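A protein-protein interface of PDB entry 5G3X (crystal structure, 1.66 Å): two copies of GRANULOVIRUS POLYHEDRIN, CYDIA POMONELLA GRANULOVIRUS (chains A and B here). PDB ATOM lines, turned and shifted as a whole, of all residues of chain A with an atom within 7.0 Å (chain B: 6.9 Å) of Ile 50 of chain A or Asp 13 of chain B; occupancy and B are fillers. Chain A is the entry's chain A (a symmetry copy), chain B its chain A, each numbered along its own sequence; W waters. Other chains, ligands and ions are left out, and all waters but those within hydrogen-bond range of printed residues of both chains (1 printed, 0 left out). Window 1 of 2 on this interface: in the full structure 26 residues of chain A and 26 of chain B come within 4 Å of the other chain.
Water W1 bridges O of Asp 54 of chain A and OG of Ser 26 of chain B.
No position is printed for both chains.
Hydrophobic or aromatic side chains of chain B that line the printed part of chain A: Leu 27.
Of the 11 printed residues of chain A, 4 touch a printed residue of chain B.
Printed residues of chain A that touch a printed residue of chain B: Glu 43, Ile 50, Ala 53 and Asp 54.
Along chain A the printed residues that touch a printed residue of chain B span positions 43 to 54.
Among the printed residues, Asp or Glu carboxylates within 4 Å of a Lys or Arg side-chain nitrogen of the other chain: Glu 43 of chain A with Arg 35 of chain B (3.1 Å).
Of the printed residues of chain B, Ala 53 of chain A touches Leu 27 (3.4 Å) and Gly 28 (3.5 Å).
Printed residues of chain B within 4 Å of Asp 54 of chain A: Asp 13, Gly 14, Ser 26, Leu 27, Gly 28 and Ala 29.
Gln 55 of chain A touches none of the printed residues of chain B.
Asp 13 of chain B touches two residues of chain A.
Of the printed residues of chain A, Leu 27 of chain B touches Ala 53 and Asp 54.
Of the printed residues of chain A, Arg 35 of chain B touches Glu 43 (3.1 Å).
The nearest residue of chain B that does not touch Ile 50 of chain A is Asn 32 of chain B (4.1 Å).
The nearest residue of chain A that does not touch Asp 13 of chain B is Asp 51 of chain A (5.7 Å).
The side-chain carboxylate (OD1) of Asp 54 of chain A sits at hydrogen-bond distance from the backbone NH (N) of Gly 28 of chain B.
OE2 of Glu 43 of chain A is in salt-bridge range of NH2 of Arg 35 of chain B (3.1 Å).
N of Gly 14 of chain B lies within hydrogen-bond range of OD2 of Asp 54 of chain A (3.3 Å).
The backbone NH (N) of Ala 29 of chain B lies within hydrogen-bond range of the side-chain carboxylate (OD1) of Asp 54 of chain A (3.0 Å).
The side-chain carboxylate of Asp 54 of chain A sits close to the side-chain carboxylate of Asp 13 of chain B (2.6 Å).
The backbone NH (N) of Thr 15 of chain B is in hydrogen-bond range of the side-chain hydroxyl (OG) of Ser 26 of chain B (2.7 Å).
OD2 of Asp 13 of chain B lies within hydrogen-bond range of N of Ala 29 of chain B (3.2 Å).
The guanidinium group (NH2) of Arg 35 of chain B is in hydrogen-bond range of the side-chain amide oxygen (OD1) of Asn 32 of chain B (2.8 Å).
Among the printed residues, pairs that only touch across the chains: Ile 50 of chain A with Asp 13 of chain B (3.3 Å), Ile 50 of chain A with Gly 28 of chain B (3.8 Å), Ala 53 of chain A with Leu 27 of chain B (3.4 Å), Ala 53 of chain A with Gly 28 of chain B (3.5 Å), Asp 54 of chain A with Ser 26 of chain B (3.2 Å) and Asp 54 of chain A with Leu 27 of chain B (3.9 Å).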
ATOM      1  N   GLU A  43      10.054  -3.098  -5.429  1.00  0.00           N
ATOM      2  CA  GLU A  43       8.985  -4.070  -5.631  1.00  0.00           C
ATOM      3  C   GLU A  43       9.494  -5.311  -6.356  1.00  0.00           C
ATOM      4  O   GLU A  43       9.158  -6.441  -5.982  1.00  0.00           O
ATOM      5  CB  GLU A  43       7.842  -3.423  -6.419  1.00  0.00           C
ATOM      6  CG  GLU A  43       6.608  -4.298  -6.597  1.00  0.00           C
ATOM      7  CD  GLU A  43       5.464  -3.563  -7.277  1.00  0.00           C
ATOM      8  OE1 GLU A  43       5.715  -2.496  -7.880  1.00  0.00           O
ATOM      9  OE2 GLU A  43       4.314  -4.051  -7.205  1.00  0.00           O
ATOM     10  N   TYR A  46      11.759  -7.736  -4.168  1.00  0.00           N
ATOM     11  CA  TYR A  46      11.058  -8.579  -3.209  1.00  0.00           C
ATOM     12  C   TYR A  46       9.844  -9.270  -3.817  1.00  0.00           C
ATOM     13  O   TYR A  46       9.113  -9.960  -3.101  1.00  0.00           O
ATOM     14  CB  TYR A  46      10.659  -7.742  -1.992  1.00  0.00           C
ATOM     15  CG  TYR A  46      11.871  -7.248  -1.226  1.00  0.00           C
ATOM     16  CD1 TYR A  46      12.613  -8.118  -0.439  1.00  0.00           C
ATOM     17  CD2 TYR A  46      12.286  -5.923  -1.307  1.00  0.00           C
ATOM     18  CE1 TYR A  46      13.726  -7.689   0.255  1.00  0.00           C
ATOM     19  CE2 TYR A  46      13.403  -5.481  -0.613  1.00  0.00           C
ATOM     20  CZ  TYR A  46      14.118  -6.371   0.167  1.00  0.00           C
ATOM     21  OH  TYR A  46      15.230  -5.955   0.866  1.00  0.00           O
ATOM     22  N   GLU A  47       9.636  -9.136  -5.126  1.00  0.00           N
ATOM     23  CA  GLU A  47       8.551  -9.860  -5.775  1.00  0.00           C
ATOM     24  C   GLU A  47       8.609 -11.367  -5.534  1.00  0.00           C
ATOM     25  O   GLU A  47       7.533 -11.984  -5.447  1.00  0.00           O
ATOM     26  CB  GLU A  47       8.564  -9.571  -7.282  1.00  0.00           C
ATOM     27  CG  GLU A  47       7.287  -9.970  -7.995  1.00  0.00           C
ATOM     28  CD  GLU A  47       7.387  -9.789  -9.497  1.00  0.00           C
ATOM     29  OE1 GLU A  47       8.462  -9.366  -9.969  1.00  0.00           O
ATOM     30  OE2 GLU A  47       6.394 -10.070 -10.203  1.00  0.00           O
ATOM     31  N   PRO A  48       9.774 -12.010  -5.427  1.00  0.00           N
ATOM     32  CA  PRO A  48       9.769 -13.450  -5.127  1.00  0.00           C
ATOM     33  C   PRO A  48       8.990 -13.807  -3.873  1.00  0.00           C
ATOM     34  O   PRO A  48       8.515 -14.944  -3.769  1.00  0.00           O
ATOM     35  CB  PRO A  48      11.259 -13.782  -4.978  1.00  0.00           C
ATOM     36  CG  PRO A  48      11.960 -12.752  -5.780  1.00  0.00           C
ATOM     37  CD  PRO A  48      11.139 -11.506  -5.665  1.00  0.00           C
ATOM     38  N   ILE A  49       8.840 -12.889  -2.911  1.00  0.00           N
ATOM     39  CA  ILE A  49       8.097 -13.250  -1.702  1.00  0.00           C
ATOM     40  C   ILE A  49       6.610 -13.317  -1.997  1.00  0.00           C
ATOM     41  O   ILE A  49       5.875 -14.064  -1.342  1.00  0.00           O
ATOM     42  CB  ILE A  49       8.375 -12.278  -0.531  1.00  0.00           C
ATOM     43  CG1 ILE A  49       7.469 -11.038  -0.590  1.00  0.00           C
ATOM     44  CG2 ILE A  49       9.857 -11.898  -0.480  1.00  0.00           C
ATOM     45  CD1 ILE A  49       7.591 -10.138   0.618  1.00  0.00           C
ATOM     46  N   ILE A  50       6.129 -12.524  -2.952  1.00  0.00           N
ATOM     47  CA  ILE A  50       4.717 -12.591  -3.307  1.00  0.00           C
ATOM     48  C   ILE A  50       4.383 -13.983  -3.828  1.00  0.00           C
ATOM     49  O   ILE A  50       3.329 -14.550  -3.513  1.00  0.00           O
ATOM     50  CB  ILE A  50       4.370 -11.490  -4.328  1.00  0.00           C
ATOM     51  CG1 ILE A  50       4.701 -10.101  -3.760  1.00  0.00           C
ATOM     52  CG2 ILE A  50       2.893 -11.559  -4.729  1.00  0.00           C
ATOM     53  CD1 ILE A  50       3.927  -9.732  -2.498  1.00  0.00           C
ATOM     54  N   ASP A  51       5.291 -14.572  -4.608  1.00  0.00           N
ATOM     55  CA  ASP A  51       5.046 -15.913  -5.124  1.00  0.00           C
ATOM     56  C   ASP A  51       5.000 -16.947  -4.008  1.00  0.00           C
ATOM     57  O   ASP A  51       4.253 -17.927  -4.105  1.00  0.00           O
ATOM     58  CB  ASP A  51       6.109 -16.282  -6.156  1.00  0.00           C
ATOM     59  CG  ASP A  51       5.536 -17.057  -7.328  1.00  0.00           C
ATOM     60  OD1 ASP A  51       4.297 -17.051  -7.493  1.00  0.00           O
ATOM     61  OD2 ASP A  51       6.322 -17.659  -8.090  1.00  0.00           O
ATOM     62  N   ILE A  52       5.780 -16.758  -2.944  1.00  0.00           N
ATOM     63  CA  ILE A  52       5.671 -17.648  -1.791  1.00  0.00           C
ATOM     64  C   ILE A  52       4.305 -17.490  -1.136  1.00  0.00           C
ATOM     65  O   ILE A  52       3.647 -18.473  -0.779  1.00  0.00           O
ATOM     66  CB  ILE A  52       6.807 -17.373  -0.793  1.00  0.00           C
ATOM     67  CG1 ILE A  52       8.167 -17.655  -1.438  1.00  0.00           C
ATOM     68  CG2 ILE A  52       6.608 -18.188   0.492  1.00  0.00           C
ATOM     69  CD1 ILE A  52       8.353 -19.080  -1.968  1.00  0.00           C
ATOM     70  N   ALA A  53       3.864 -16.251  -0.953  1.00  0.00           N
ATOM     71  CA  ALA A  53       2.548 -16.014  -0.381  1.00  0.00           C
ATOM     72  C   ALA A  53       1.446 -16.547  -1.286  1.00  0.00           C
ATOM     73  O   ALA A  53       0.409 -17.006  -0.791  1.00  0.00           O
ATOM     74  CB  ALA A  53       2.366 -14.519  -0.126  1.00  0.00           C
ATOM     75  N   ASP A  54       1.662 -16.522  -2.605  1.00  0.00           N
ATOM     76  CA  ASP A  54       0.656 -16.966  -3.560  1.00  0.00           C
ATOM     77  C   ASP A  54       0.521 -18.479  -3.627  1.00  0.00           C
ATOM     78  O   ASP A  54      -0.318 -18.967  -4.394  1.00  0.00           O
ATOM     79  CB  ASP A  54       0.968 -16.445  -4.962  1.00  0.00           C
ATOM     80  CG  ASP A  54       0.522 -15.015  -5.168  1.00  0.00           C
ATOM     81  OD1 ASP A  54      -0.242 -14.493  -4.337  1.00  0.00           O
ATOM     82  OD2 ASP A  54       0.937 -14.417  -6.175  1.00  0.00           O
ATOM     83  N   GLN A  55       1.322 -19.228  -2.866  1.00  0.00           N
ATOM     84  CA  GLN A  55       1.042 -20.645  -2.699  1.00  0.00           C
ATOM     85  C   GLN A  55      -0.253 -20.859  -1.931  1.00  0.00           C
ATOM     86  O   GLN A  55      -0.760 -21.983  -1.903  1.00  0.00           O
ATOM     87  CB  GLN A  55       2.206 -21.347  -1.983  1.00  0.00           C
ATOM     88  CG  GLN A  55       2.102 -22.877  -1.940  1.00  0.00           C
ATOM     89  CD  GLN A  55       2.209 -23.536  -3.312  1.00  0.00           C
ATOM     90  OE1 GLN A  55       2.657 -22.919  -4.288  1.00  0.00           O
ATOM     91  NE2 GLN A  55       1.809 -24.808  -3.389  1.00  0.00           N
ATOM     92  N   HIS B  12       0.316  -9.377 -12.344  1.00  0.00           N
ATOM     93  CA  HIS B  12      -0.554 -10.486 -12.730  1.00  0.00           C
ATOM     94  C   HIS B  12      -0.240 -11.743 -11.925  1.00  0.00           C
ATOM     95  O   HIS B  12      -0.327 -12.852 -12.442  1.00  0.00           O
ATOM     96  CB  HIS B  12      -0.417 -10.785 -14.226  1.00  0.00           C
ATOM     97  N   ASP B  13       0.122 -11.575 -10.658  1.00  0.00           N
ATOM     98  CA  ASP B  13       0.435 -12.725  -9.826  1.00  0.00           C
ATOM     99  C   ASP B  13      -0.846 -13.353  -9.292  1.00  0.00           C
ATOM    100  O   ASP B  13      -1.872 -12.687  -9.125  1.00  0.00           O
ATOM    101  CB  ASP B  13       1.337 -12.323  -8.661  1.00  0.00           C
ATOM    102  CG  ASP B  13       0.624 -11.438  -7.653  1.00  0.00           C
ATOM    103  OD1 ASP B  13       0.461 -10.228  -7.927  1.00  0.00           O
ATOM    104  OD2 ASP B  13       0.219 -11.957  -6.589  1.00  0.00           O
ATOM    105  N   GLY B  14      -0.782 -14.652  -9.027  1.00  0.00           N
ATOM    106  CA  GLY B  14      -1.907 -15.299  -8.384  1.00  0.00           C
ATOM    107  C   GLY B  14      -3.070 -15.505  -9.340  1.00  0.00           C
ATOM    108  O   GLY B  14      -2.961 -15.354 -10.560  1.00  0.00           O
ATOM    109  N   THR B  15      -4.216 -15.830  -8.752  1.00  0.00           N
ATOM    110  CA  THR B  15      -5.350 -16.301  -9.539  1.00  0.00           C
ATOM    111  C   THR B  15      -6.596 -16.311  -8.665  1.00  0.00           C
ATOM    112  O   THR B  15      -6.575 -15.909  -7.499  1.00  0.00           O
ATOM    113  CB  THR B  15      -5.074 -17.688 -10.124  1.00  0.00           C
ATOM    114  OG1 THR B  15      -6.000 -17.959 -11.189  1.00  0.00           O
ATOM    115  CG2 THR B  15      -5.189 -18.775  -9.057  1.00  0.00           C
ATOM    116  N   LYS B  25      -8.926 -16.178  -3.636  1.00  0.00           N
ATOM    117  CA  LYS B  25      -7.944 -15.354  -4.315  1.00  0.00           C
ATOM    118  C   LYS B  25      -6.591 -15.554  -3.647  1.00  0.00           C
ATOM    119  O   LYS B  25      -6.510 -15.769  -2.439  1.00  0.00           O
ATOM    120  CB  LYS B  25      -8.329 -13.876  -4.277  1.00  0.00           C
ATOM    121  CG  LYS B  25      -7.410 -12.994  -5.092  1.00  0.00           C
ATOM    122  CD  LYS B  25      -7.893 -11.556  -5.134  1.00  0.00           C
ATOM    123  CE  LYS B  25      -6.897 -10.656  -5.848  1.00  0.00           C
ATOM    124  NZ  LYS B  25      -7.340  -9.238  -5.814  1.00  0.00           N
ATOM    125  N   SER B  26      -5.535 -15.476  -4.451  1.00  0.00           N
ATOM    126  CA  SER B  26      -4.179 -15.699  -3.970  1.00  0.00           C
ATOM    127  C   SER B  26      -3.818 -14.727  -2.853  1.00  0.00           C
ATOM    128  O   SER B  26      -4.074 -13.526  -2.954  1.00  0.00           O
ATOM    129  CB  SER B  26      -3.193 -15.538  -5.125  1.00  0.00           C
ATOM    130  OG  SER B  26      -3.541 -16.361  -6.220  1.00  0.00           O
ATOM    131  N   LEU B  27      -3.200 -15.256  -1.794  1.00  0.00           N
ATOM    132  CA  LEU B  27      -2.870 -14.451  -0.623  1.00  0.00           C
ATOM    133  C   LEU B  27      -1.868 -13.346  -0.947  1.00  0.00           C
ATOM    134  O   LEU B  27      -1.994 -12.220  -0.451  1.00  0.00           O
ATOM    135  CB  LEU B  27      -2.323 -15.357   0.478  1.00  0.00           C
ATOM    136  CG  LEU B  27      -1.751 -14.660   1.709  1.00  0.00           C
ATOM    137  CD1 LEU B  27      -2.834 -13.896   2.459  1.00  0.00           C
ATOM    138  CD2 LEU B  27      -1.098 -15.672   2.611  1.00  0.00           C
ATOM    139  N   GLY B  28      -0.852 -13.644  -1.754  1.00  0.00           N
ATOM    140  CA  GLY B  28       0.136 -12.620  -2.065  1.00  0.00           C
ATOM    141  C   GLY B  28      -0.460 -11.464  -2.844  1.00  0.00           C
ATOM    142  O   GLY B  28      -0.142 -10.297  -2.590  1.00  0.00           O
ATOM    143  N   ALA B  29      -1.317 -11.776  -3.812  1.00  0.00           N
ATOM    144  CA  ALA B  29      -2.055 -10.749  -4.537  1.00  0.00           C
ATOM    145  C   ALA B  29      -2.885  -9.880  -3.593  1.00  0.00           C
ATOM    146  O   ALA B  29      -2.888  -8.650  -3.718  1.00  0.00           O
ATOM    147  CB  ALA B  29      -2.942 -11.413  -5.591  1.00  0.00           C
ATOM    148  N   VAL B  30      -3.584 -10.494  -2.631  1.00  0.00           N
ATOM    149  CA  VAL B  30      -4.387  -9.720  -1.684  1.00  0.00           C
ATOM    150  C   VAL B  30      -3.492  -8.835  -0.825  1.00  0.00           C
ATOM    151  O   VAL B  30      -3.773  -7.649  -0.632  1.00  0.00           O
ATOM    152  CB  VAL B  30      -5.261 -10.646  -0.819  1.00  0.00           C
ATOM    153  CG1 VAL B  30      -5.908  -9.867   0.319  1.00  0.00           C
ATOM    154  CG2 VAL B  30      -6.336 -11.290  -1.661  1.00  0.00           C
ATOM    155  N   LEU B  31      -2.410  -9.399  -0.283  1.00  0.00           N
ATOM    156  CA  LEU B  31      -1.501  -8.586   0.518  1.00  0.00           C
ATOM    157  C   LEU B  31      -0.879  -7.473  -0.315  1.00  0.00           C
ATOM    158  O   LEU B  31      -0.610  -6.382   0.204  1.00  0.00           O
ATOM    159  CB  LEU B  31      -0.417  -9.469   1.144  1.00  0.00           C
ATOM    160  CG  LEU B  31      -0.901 -10.487   2.180  1.00  0.00           C
ATOM    161  CD1 LEU B  31       0.257 -11.354   2.653  1.00  0.00           C
ATOM    162  CD2 LEU B  31      -1.568  -9.807   3.357  1.00  0.00           C
ATOM    163  N   ASN B  32      -0.665  -7.719  -1.609  1.00  0.00           N
ATOM    164  CA  ASN B  32      -0.170  -6.670  -2.496  1.00  0.00           C
ATOM    165  C   ASN B  32      -1.221  -5.586  -2.707  1.00  0.00           C
ATOM    166  O   ASN B  32      -0.893  -4.394  -2.734  1.00  0.00           O
ATOM    167  CB  ASN B  32       0.254  -7.274  -3.833  1.00  0.00           C
ATOM    168  CG  ASN B  32       1.312  -6.450  -4.528  1.00  0.00           C
ATOM    169  OD1 ASN B  32       2.411  -6.276  -4.005  1.00  0.00           O
ATOM    170  ND2 ASN B  32       0.992  -5.939  -5.711  1.00  0.00           N
ATOM    171  N   ARG B  35      -1.028  -3.528   0.375  1.00  0.00           N
ATOM    172  CA  ARG B  35       0.172  -2.696   0.381  1.00  0.00           C
ATOM    173  C   ARG B  35       0.027  -1.521  -0.580  1.00  0.00           C
ATOM    174  O   ARG B  35       0.384  -0.386  -0.246  1.00  0.00           O
ATOM    175  CB  ARG B  35       1.398  -3.542   0.020  1.00  0.00           C
ATOM    176  CG  ARG B  35       2.723  -2.773   0.039  1.00  0.00           C
ATOM    177  CD  ARG B  35       3.885  -3.606  -0.488  1.00  0.00           C
ATOM    178  NE  ARG B  35       3.684  -4.042  -1.869  1.00  0.00           N
ATOM    179  CZ  ARG B  35       3.882  -3.275  -2.939  1.00  0.00           C
ATOM    180  NH1 ARG B  35       4.280  -2.017  -2.801  1.00  0.00           N
ATOM    181  NH2 ARG B  35       3.675  -3.767  -4.153  1.00  0.00           N
HETATM  182  O   HOH W   1      -2.575 -18.672  -5.520  1.00  0.00           O
